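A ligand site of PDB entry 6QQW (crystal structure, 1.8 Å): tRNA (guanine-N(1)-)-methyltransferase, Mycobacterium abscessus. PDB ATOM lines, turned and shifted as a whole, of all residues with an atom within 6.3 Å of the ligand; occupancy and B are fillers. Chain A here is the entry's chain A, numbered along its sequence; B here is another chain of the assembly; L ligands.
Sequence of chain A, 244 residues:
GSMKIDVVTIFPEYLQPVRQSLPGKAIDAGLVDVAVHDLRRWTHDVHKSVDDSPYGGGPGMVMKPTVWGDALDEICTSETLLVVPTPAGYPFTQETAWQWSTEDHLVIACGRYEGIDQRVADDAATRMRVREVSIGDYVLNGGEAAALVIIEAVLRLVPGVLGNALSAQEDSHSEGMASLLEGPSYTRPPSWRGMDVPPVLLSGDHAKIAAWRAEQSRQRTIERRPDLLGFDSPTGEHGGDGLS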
ATOM      1  N   PRO A  85      10.123  15.845   4.188  1.00  0.00           N
ATOM      2  CA  PRO A  85       9.728  14.448   4.400  1.00  0.00           C
ATOM      3  C   PRO A  85       8.372  14.354   5.092  1.00  0.00           C
ATOM      4  O   PRO A  85       8.051  15.158   5.969  1.00  0.00           O
ATOM      5  CB  PRO A  85      10.866  13.881   5.262  1.00  0.00           C
ATOM      6  CG  PRO A  85      12.062  14.751   4.935  1.00  0.00           C
ATOM      7  CD  PRO A  85      11.476  16.135   4.712  1.00  0.00           C
ATOM      8  N   THR A  86       7.569  13.380   4.660  1.00  0.00           N
ATOM      9  CA  THR A  86       6.250  13.152   5.259  1.00  0.00           C
ATOM     10  C   THR A  86       5.723  11.807   4.807  1.00  0.00           C
ATOM     11  O   THR A  86       5.955  11.387   3.674  1.00  0.00           O
ATOM     12  CB  THR A  86       5.226  14.265   4.914  1.00  0.00           C
ATOM     13  OG1 THR A  86       3.891  13.794   5.178  1.00  0.00           O
ATOM     14  CG2 THR A  86       5.340  14.725   3.461  1.00  0.00           C
ATOM     15  N   PRO A  87       5.017  11.102   5.701  1.00  0.00           N
ATOM     16  CA  PRO A  87       4.477   9.797   5.308  1.00  0.00           C
ATOM     17  C   PRO A  87       3.425   9.954   4.211  1.00  0.00           C
ATOM     18  O   PRO A  87       3.121   8.981   3.535  1.00  0.00           O
ATOM     19  CB  PRO A  87       3.872   9.247   6.615  1.00  0.00           C
ATOM     20  CG  PRO A  87       3.701  10.410   7.500  1.00  0.00           C
ATOM     21  CD  PRO A  87       4.661  11.486   7.085  1.00  0.00           C
ATOM     22  N   ALA A  88       2.908  11.164   4.042  1.00  0.00           N
ATOM     23  CA  ALA A  88       1.907  11.436   3.013  1.00  0.00           C
ATOM     24  C   ALA A  88       2.503  12.050   1.749  1.00  0.00           C
ATOM     25  O   ALA A  88       1.785  12.633   0.933  1.00  0.00           O
ATOM     26  CB  ALA A  88       0.822  12.365   3.568  1.00  0.00           C
ATOM     27  N   CYS A 110      12.715  18.986   8.562  1.00  0.00           N
ATOM     28  CA  CYS A 110      12.346  17.781   9.310  1.00  0.00           C
ATOM     29  C   CYS A 110      11.272  18.038  10.353  1.00  0.00           C
ATOM     30  O   CYS A 110      11.490  18.786  11.307  1.00  0.00           O
ATOM     31  CB  CYS A 110      13.596  17.203  10.004  1.00  0.00           C
ATOM     32  SG  CYS A 110      14.898  16.689   8.849  1.00  0.00           S
ATOM     33  N   GLY A 111      10.101  17.421  10.155  1.00  0.00           N
ATOM     34  CA  GLY A 111       9.021  17.507  11.125  1.00  0.00           C
ATOM     35  C   GLY A 111       9.172  16.521  12.256  1.00  0.00           C
ATOM     36  O   GLY A 111       9.968  15.584  12.178  1.00  0.00           O
ATOM     37  N   ARG A 112       8.393  16.744  13.318  1.00  0.00           N
ATOM     38  CA  ARG A 112       8.229  15.784  14.409  1.00  0.00           C
ATOM     39  C   ARG A 112       6.761  15.838  14.816  1.00  0.00           C
ATOM     40  O   ARG A 112       5.961  16.470  14.121  1.00  0.00           O
ATOM     41  CB  ARG A 112       9.148  16.108  15.583  1.00  0.00           C
ATOM     42  CG  ARG A 112      10.582  15.607  15.414  1.00  0.00           C
ATOM     43  CD  ARG A 112      10.722  14.173  15.935  1.00  0.00           C
ATOM     44  NE  ARG A 112      11.860  13.490  15.324  1.00  0.00           N
ATOM     45  CZ  ARG A 112      12.267  12.275  15.670  1.00  0.00           C
ATOM     46  NH1 ARG A 112      11.627  11.613  16.632  1.00  0.00           N
ATOM     47  NH2 ARG A 112      13.300  11.714  15.057  1.00  0.00           N
ATOM     48  N   TYR A 113       6.393  15.173  15.916  1.00  0.00           N
ATOM     49  CA  TYR A 113       4.998  15.127  16.350  1.00  0.00           C
ATOM     50  C   TYR A 113       4.127  14.597  15.214  1.00  0.00           C
ATOM     51  O   TYR A 113       4.482  13.618  14.584  1.00  0.00           O
ATOM     52  CB  TYR A 113       4.533  16.513  16.832  1.00  0.00           C
ATOM     53  CG  TYR A 113       5.458  17.128  17.866  1.00  0.00           C
ATOM     54  CD1 TYR A 113       5.273  16.881  19.218  1.00  0.00           C
ATOM     55  CD2 TYR A 113       6.514  17.951  17.485  1.00  0.00           C
ATOM     56  CE1 TYR A 113       6.105  17.433  20.169  1.00  0.00           C
ATOM     57  CE2 TYR A 113       7.362  18.510  18.433  1.00  0.00           C
ATOM     58  CZ  TYR A 113       7.147  18.242  19.779  1.00  0.00           C
ATOM     59  OH  TYR A 113       7.979  18.793  20.730  1.00  0.00           O
ATOM     60  N   GLU A 114       3.012  15.268  14.921  1.00  0.00           N
ATOM     61  CA  GLU A 114       2.156  14.844  13.815  1.00  0.00           C
ATOM     62  C   GLU A 114       2.448  15.553  12.498  1.00  0.00           C
ATOM     63  O   GLU A 114       1.725  15.375  11.520  1.00  0.00           O
ATOM     64  CB  GLU A 114       0.679  15.060  14.177  1.00  0.00           C
ATOM     65  CG  GLU A 114       0.244  14.258  15.385  1.00  0.00           C
ATOM     66  CD  GLU A 114       0.348  12.762  15.133  1.00  0.00           C
ATOM     67  OE1 GLU A 114       1.415  12.187  15.418  1.00  0.00           O
ATOM     68  OE2 GLU A 114      -0.650  12.175  14.658  1.00  0.00           O
ATOM     69  N   GLY A 115       3.507  16.347  12.452  1.00  0.00           N
ATOM     70  CA  GLY A 115       3.885  16.992  11.209  1.00  0.00           C
ATOM     71  C   GLY A 115       3.865  18.502  11.310  1.00  0.00           C
ATOM     72  O   GLY A 115       3.724  19.053  12.398  1.00  0.00           O
ATOM     73  N   ILE A 116       3.996  19.167  10.173  1.00  0.00           N
ATOM     74  CA  ILE A 116       4.086  20.632  10.142  1.00  0.00           C
ATOM     75  C   ILE A 116       2.784  21.233   9.619  1.00  0.00           C
ATOM     76  O   ILE A 116       2.205  20.705   8.684  1.00  0.00           O
ATOM     77  CB  ILE A 116       5.249  21.096   9.262  1.00  0.00           C
ATOM     78  CG1 ILE A 116       6.532  20.374   9.675  1.00  0.00           C
ATOM     79  CG2 ILE A 116       5.396  22.616   9.310  1.00  0.00           C
ATOM     80  CD1 ILE A 116       7.715  20.646   8.759  1.00  0.00           C
ATOM     81  N   VAL A 133       7.795  14.508   0.333  1.00  0.00           N
ATOM     82  CA  VAL A 133       8.197  13.186  -0.148  1.00  0.00           C
ATOM     83  C   VAL A 133       8.198  12.154   0.968  1.00  0.00           C
ATOM     84  O   VAL A 133       8.517  12.473   2.106  1.00  0.00           O
ATOM     85  CB  VAL A 133       9.592  13.187  -0.801  1.00  0.00           C
ATOM     86  CG1 VAL A 133       9.568  13.936  -2.133  1.00  0.00           C
ATOM     87  CG2 VAL A 133      10.642  13.801   0.150  1.00  0.00           C
ATOM     88  N   SER A 134       7.845  10.934   0.601  1.00  0.00           N
ATOM     89  CA  SER A 134       7.893   9.785   1.502  1.00  0.00           C
ATOM     90  C   SER A 134       9.047   8.907   1.051  1.00  0.00           C
ATOM     91  O   SER A 134       9.241   8.730  -0.174  1.00  0.00           O
ATOM     92  CB  SER A 134       6.572   9.013   1.473  1.00  0.00           C
ATOM     93  OG  SER A 134       6.710   7.716   2.047  1.00  0.00           O
ATOM     94  N   ILE A 135       9.798   8.320   1.978  1.00  0.00           N
ATOM     95  CA  ILE A 135      10.870   7.394   1.550  1.00  0.00           C
ATOM     96  C   ILE A 135      10.460   5.913   1.573  1.00  0.00           C
ATOM     97  O   ILE A 135      11.278   5.027   1.264  1.00  0.00           O
ATOM     98  CB  ILE A 135      12.142   7.546   2.417  1.00  0.00           C
ATOM     99  CG1 ILE A 135      11.853   7.245   3.892  1.00  0.00           C
ATOM    100  CG2 ILE A 135      12.774   8.942   2.242  1.00  0.00           C
ATOM    101  CD1 ILE A 135      13.119   6.865   4.704  1.00  0.00           C
ATOM    102  N   GLY A 136       9.213   5.627   1.924  1.00  0.00           N
ATOM    103  CA  GLY A 136       8.732   4.248   1.877  1.00  0.00           C
ATOM    104  C   GLY A 136       7.441   4.095   2.646  1.00  0.00           C
ATOM    105  O   GLY A 136       7.018   5.048   3.320  1.00  0.00           O
ATOM    106  N   ASP A 137       6.817   2.925   2.547  1.00  0.00           N
ATOM    107  CA  ASP A 137       5.489   2.732   3.117  1.00  0.00           C
ATOM    108  C   ASP A 137       5.536   2.208   4.541  1.00  0.00           C
ATOM    109  O   ASP A 137       5.044   1.122   4.840  1.00  0.00           O
ATOM    110  CB  ASP A 137       4.659   1.812   2.237  1.00  0.00           C
ATOM    111  CG  ASP A 137       4.273   2.476   0.944  1.00  0.00           C
ATOM    112  OD1 ASP A 137       4.304   3.719   0.906  1.00  0.00           O
ATOM    113  OD2 ASP A 137       3.926   1.762  -0.020  1.00  0.00           O
ATOM    114  N   TYR A 138       6.151   3.013   5.409  1.00  0.00           N
ATOM    115  CA  TYR A 138       6.213   2.762   6.834  1.00  0.00           C
ATOM    116  C   TYR A 138       6.224   4.122   7.495  1.00  0.00           C
ATOM    117  O   TYR A 138       6.480   5.136   6.858  1.00  0.00           O
ATOM    118  CB  TYR A 138       7.464   1.964   7.206  1.00  0.00           C
ATOM    119  CG  TYR A 138       8.661   2.441   6.419  1.00  0.00           C
ATOM    120  CD1 TYR A 138       9.324   3.627   6.756  1.00  0.00           C
ATOM    121  CD2 TYR A 138       9.105   1.735   5.304  1.00  0.00           C
ATOM    122  CE1 TYR A 138      10.405   4.087   5.997  1.00  0.00           C
ATOM    123  CE2 TYR A 138      10.173   2.173   4.557  1.00  0.00           C
ATOM    124  CZ  TYR A 138      10.829   3.348   4.900  1.00  0.00           C
ATOM    125  OH  TYR A 138      11.884   3.758   4.119  1.00  0.00           O
ATOM    126  N   VAL A 139       5.955   4.151   8.800  1.00  0.00           N
ATOM    127  CA  VAL A 139       5.824   5.402   9.523  1.00  0.00           C
ATOM    128  C   VAL A 139       6.998   5.590  10.470  1.00  0.00           C
ATOM    129  O   VAL A 139       7.299   4.689  11.250  1.00  0.00           O
ATOM    130  CB  VAL A 139       4.494   5.433  10.307  1.00  0.00           C
ATOM    131  CG1 VAL A 139       4.354   6.749  11.074  1.00  0.00           C
ATOM    132  CG2 VAL A 139       3.316   5.243   9.369  1.00  0.00           C
ATOM    133  N   LEU A 140       7.670   6.736  10.374  1.00  0.00           N
ATOM    134  CA  LEU A 140       8.785   7.063  11.264  1.00  0.00           C
ATOM    135  C   LEU A 140       8.273   7.978  12.378  1.00  0.00           C
ATOM    136  O   LEU A 140       7.111   8.357  12.362  1.00  0.00           O
ATOM    137  CB  LEU A 140       9.914   7.757  10.488  1.00  0.00           C
ATOM    138  CG  LEU A 140      10.527   6.929   9.345  1.00  0.00           C
ATOM    139  CD1 LEU A 140      11.331   7.806   8.408  1.00  0.00           C
ATOM    140  CD2 LEU A 140      11.392   5.801   9.910  1.00  0.00           C
ATOM    141  N   ASN A 141       9.138   8.359  13.314  1.00  0.00           N
ATOM    142  CA  ASN A 141       8.698   9.327  14.336  1.00  0.00           C
ATOM    143  C   ASN A 141       8.887  10.787  13.882  1.00  0.00           C
ATOM    144  O   ASN A 141       8.355  11.707  14.496  1.00  0.00           O
ATOM    145  CB  ASN A 141       9.467   9.123  15.640  1.00  0.00           C
ATOM    146  CG  ASN A 141       8.881   8.039  16.495  1.00  0.00           C
ATOM    147  OD1 ASN A 141       7.650   7.859  16.558  1.00  0.00           O
ATOM    148  ND2 ASN A 141       9.742   7.295  17.166  1.00  0.00           N
ATOM    149  N   GLY A 142       9.660  10.975  12.821  1.00  0.00           N
ATOM    150  CA  GLY A 142       9.934  12.327  12.344  1.00  0.00           C
ATOM    151  C   GLY A 142      10.733  12.264  11.061  1.00  0.00           C
ATOM    152  O   GLY A 142      10.994  11.182  10.525  1.00  0.00           O
ATOM    153  N   GLY A 143      11.102  13.435  10.536  1.00  0.00           N
ATOM    154  CA  GLY A 143      11.751  13.490   9.244  1.00  0.00           C
ATOM    155  C   GLY A 143      13.243  13.213   9.202  1.00  0.00           C
ATOM    156  O   GLY A 143      13.822  13.054   8.109  1.00  0.00           O
ATOM    157  N   GLU A 144      13.875  13.153  10.376  1.00  0.00           N
ATOM    158  CA  GLU A 144      15.351  13.067  10.436  1.00  0.00           C
ATOM    159  C   GLU A 144      15.928  11.828   9.746  1.00  0.00           C
ATOM    160  O   GLU A 144      16.886  11.935   8.969  1.00  0.00           O
ATOM    161  CB  GLU A 144      15.825  13.101  11.899  1.00  0.00           C
ATOM    162  CG  GLU A 144      15.705  14.461  12.585  1.00  0.00           C
ATOM    163  CD  GLU A 144      14.286  14.802  13.010  1.00  0.00           C
ATOM    164  OE1 GLU A 144      13.409  13.909  12.984  1.00  0.00           O
ATOM    165  OE2 GLU A 144      14.054  15.983  13.360  1.00  0.00           O
ATOM    166  N   ALA A 146      14.571  10.113   7.443  1.00  0.00           N
ATOM    167  CA  ALA A 146      14.286  10.315   6.019  1.00  0.00           C
ATOM    168  C   ALA A 146      15.296  11.259   5.395  1.00  0.00           C
ATOM    169  O   ALA A 146      15.732  11.051   4.258  1.00  0.00           O
ATOM    170  CB  ALA A 146      12.869  10.840   5.817  1.00  0.00           C
ATOM    171  N   ARG B 156       8.778   2.259  17.514  1.00  0.00           N
ATOM    172  CA  ARG B 156       7.634   3.092  17.860  1.00  0.00           C
ATOM    173  C   ARG B 156       6.343   2.265  17.962  1.00  0.00           C
ATOM    174  O   ARG B 156       5.305   2.744  18.434  1.00  0.00           O
ATOM    175  CB  ARG B 156       7.489   4.232  16.854  1.00  0.00           C
ATOM    176  CG  ARG B 156       7.071   3.806  15.478  1.00  0.00           C
ATOM    177  CD  ARG B 156       7.101   5.002  14.531  1.00  0.00           C
ATOM    178  NE  ARG B 156       6.047   5.973  14.812  1.00  0.00           N
ATOM    179  CZ  ARG B 156       4.773   5.806  14.466  1.00  0.00           C
ATOM    180  NH1 ARG B 156       4.379   4.696  13.856  1.00  0.00           N
ATOM    181  NH2 ARG B 156       3.875   6.749  14.746  1.00  0.00           N
ATOM    182  N   GLU B 182      -2.251  10.523   5.173  1.00  0.00           N
ATOM    183  CA  GLU B 182      -2.647  11.571   6.120  1.00  0.00           C
ATOM    184  C   GLU B 182      -2.915  12.875   5.389  1.00  0.00           C
ATOM    185  O   GLU B 182      -2.151  13.278   4.515  1.00  0.00           O
ATOM    186  CB  GLU B 182      -1.554  11.778   7.182  1.00  0.00           C
ATOM    187  CG  GLU B 182      -1.284  10.570   8.046  1.00  0.00           C
ATOM    188  CD  GLU B 182      -2.249  10.451   9.212  1.00  0.00           C
ATOM    189  OE1 GLU B 182      -3.275  11.167   9.216  1.00  0.00           O
ATOM    190  OE2 GLU B 182      -1.983   9.646  10.132  1.00  0.00           O
HETATM  191  C1  LIG L   1       7.417  13.251   9.985  1.00  0.00           C
HETATM  192  C2  LIG L   1       4.100  11.147  11.930  1.00  0.00           C
HETATM  193  C3  LIG L   1       2.192  12.005  10.659  1.00  0.00           C
HETATM  194  C4  LIG L   1       3.363   9.999  12.285  1.00  0.00           C
HETATM  195  C5  LIG L   1       6.355  13.550  12.008  1.00  0.00           C
HETATM  196  C6  LIG L   1       7.077  14.212  11.001  1.00  0.00           C
HETATM  197  N1  LIG L   1       8.266   7.653   4.631  1.00  0.00           N
HETATM  198  C7  LIG L   1       8.034   8.247   5.901  1.00  0.00           C
HETATM  199  N2  LIG L   1       7.640   7.594   6.993  1.00  0.00           N
HETATM  200  N3  LIG L   1       7.524   8.482   7.981  1.00  0.00           N
HETATM  201  C8  LIG L   1       7.866   9.691   7.563  1.00  0.00           C
HETATM  202  C9  LIG L   1       8.159   9.611   6.256  1.00  0.00           C
HETATM  203  C10 LIG L   1       7.779  10.942   8.402  1.00  0.00           C
HETATM  204  C11 LIG L   1       8.319  12.151   7.963  1.00  0.00           C
HETATM  205  C12 LIG L   1       8.141  13.315   8.757  1.00  0.00           C
HETATM  206  C13 LIG L   1       6.890  12.065  10.413  1.00  0.00           C
HETATM  207  C14 LIG L   1       7.063  10.876   9.600  1.00  0.00           C
HETATM  208  N4  LIG L   1       6.252  12.291  11.652  1.00  0.00           N
HETATM  209  C15 LIG L   1       5.558  11.307  12.444  1.00  0.00           C
HETATM  210  C16 LIG L   1       3.514  12.158  11.130  1.00  0.00           C
HETATM  211  C17 LIG L   1       1.455  10.856  11.014  1.00  0.00           C
HETATM  212  C18 LIG L   1       2.032   9.857  11.824  1.00  0.00           C
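The backbone carbonyl oxygen of Tyr 138 sits at hydrogen-bond distance from a nitrogen (N2) of the ligand. N of Leu 140 lies within hydrogen-bond range of N3 of the ligand (3.0 Å). A nitrogen (N1) of the ligand lies within hydrogen-bond range of the side-chain hydroxyl (OG) of Ser 134 (3.0 Å). The backbone carbonyl oxygen (O) of Gly 136 sits at hydrogen-bond distance from a nitrogen (N1) of the ligand (3.2 Å).
The side-chain hydroxyl (OH) of Tyr 138 lies within hydrogen-bond range of the backbone carbonyl oxygen (O) of Ile 135. OG of Ser 134 lies within hydrogen-bond range of O of Gly 136 (3.0 Å). The backbone NH of Gly 143 is in hydrogen-bond range of the backbone carbonyl oxygen of Gly 111 (2.9 Å). OD1 of Asn 141 is in hydrogen-bond range of NE of Arg 156 of chain B, at 3.0 Å. The backbone carbonyl oxygen of Val 133 sits at hydrogen-bond distance from the backbone NH of Thr 86 (2.9 Å). OG1 of Thr 86 sits close to N of Ala 88. The side-chain carboxylate (OE1) of Glu 144 lies within salt-bridge range of the guanidinium group (NE) of Arg 112, at 2.8 Å.
N of Ile 135 lies close to N1 of the ligand, 3.1 Å away. Pro 85 touches the ligand. Thr 86 touches the ligand. CD of Pro 87 touches C10 of the ligand (3.4 Å). Gly 111 touches the ligand. O of Arg 112 touches C5 of the ligand, at 3.6 Å. Tyr 113 touches the ligand. O of Glu 114 touches C3 of the ligand, 3.5 Å away. CG1 of Val 139 touches C4 of the ligand, 3.6 Å away. Asn 141 touches the ligand (O to C15, 3.5 Å). CA of Gly 142 touches C1 of the ligand, 3.6 Å away. N of Gly 143 touches C12 of the ligand, at 3.5 Å. OE2 of Glu 182 of chain B touches C17 of the ligand (3.7 Å). Hydrophobic or aromatic side chains within 4 Å of the ligand: Pro 87, Ile 135, Val 139 and Leu 140. Of the 26 residues printed, 17 come within 4 Å of the ligand. The nearest printed residue that does not touch the ligand is Gly 115 (4.02 Å).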
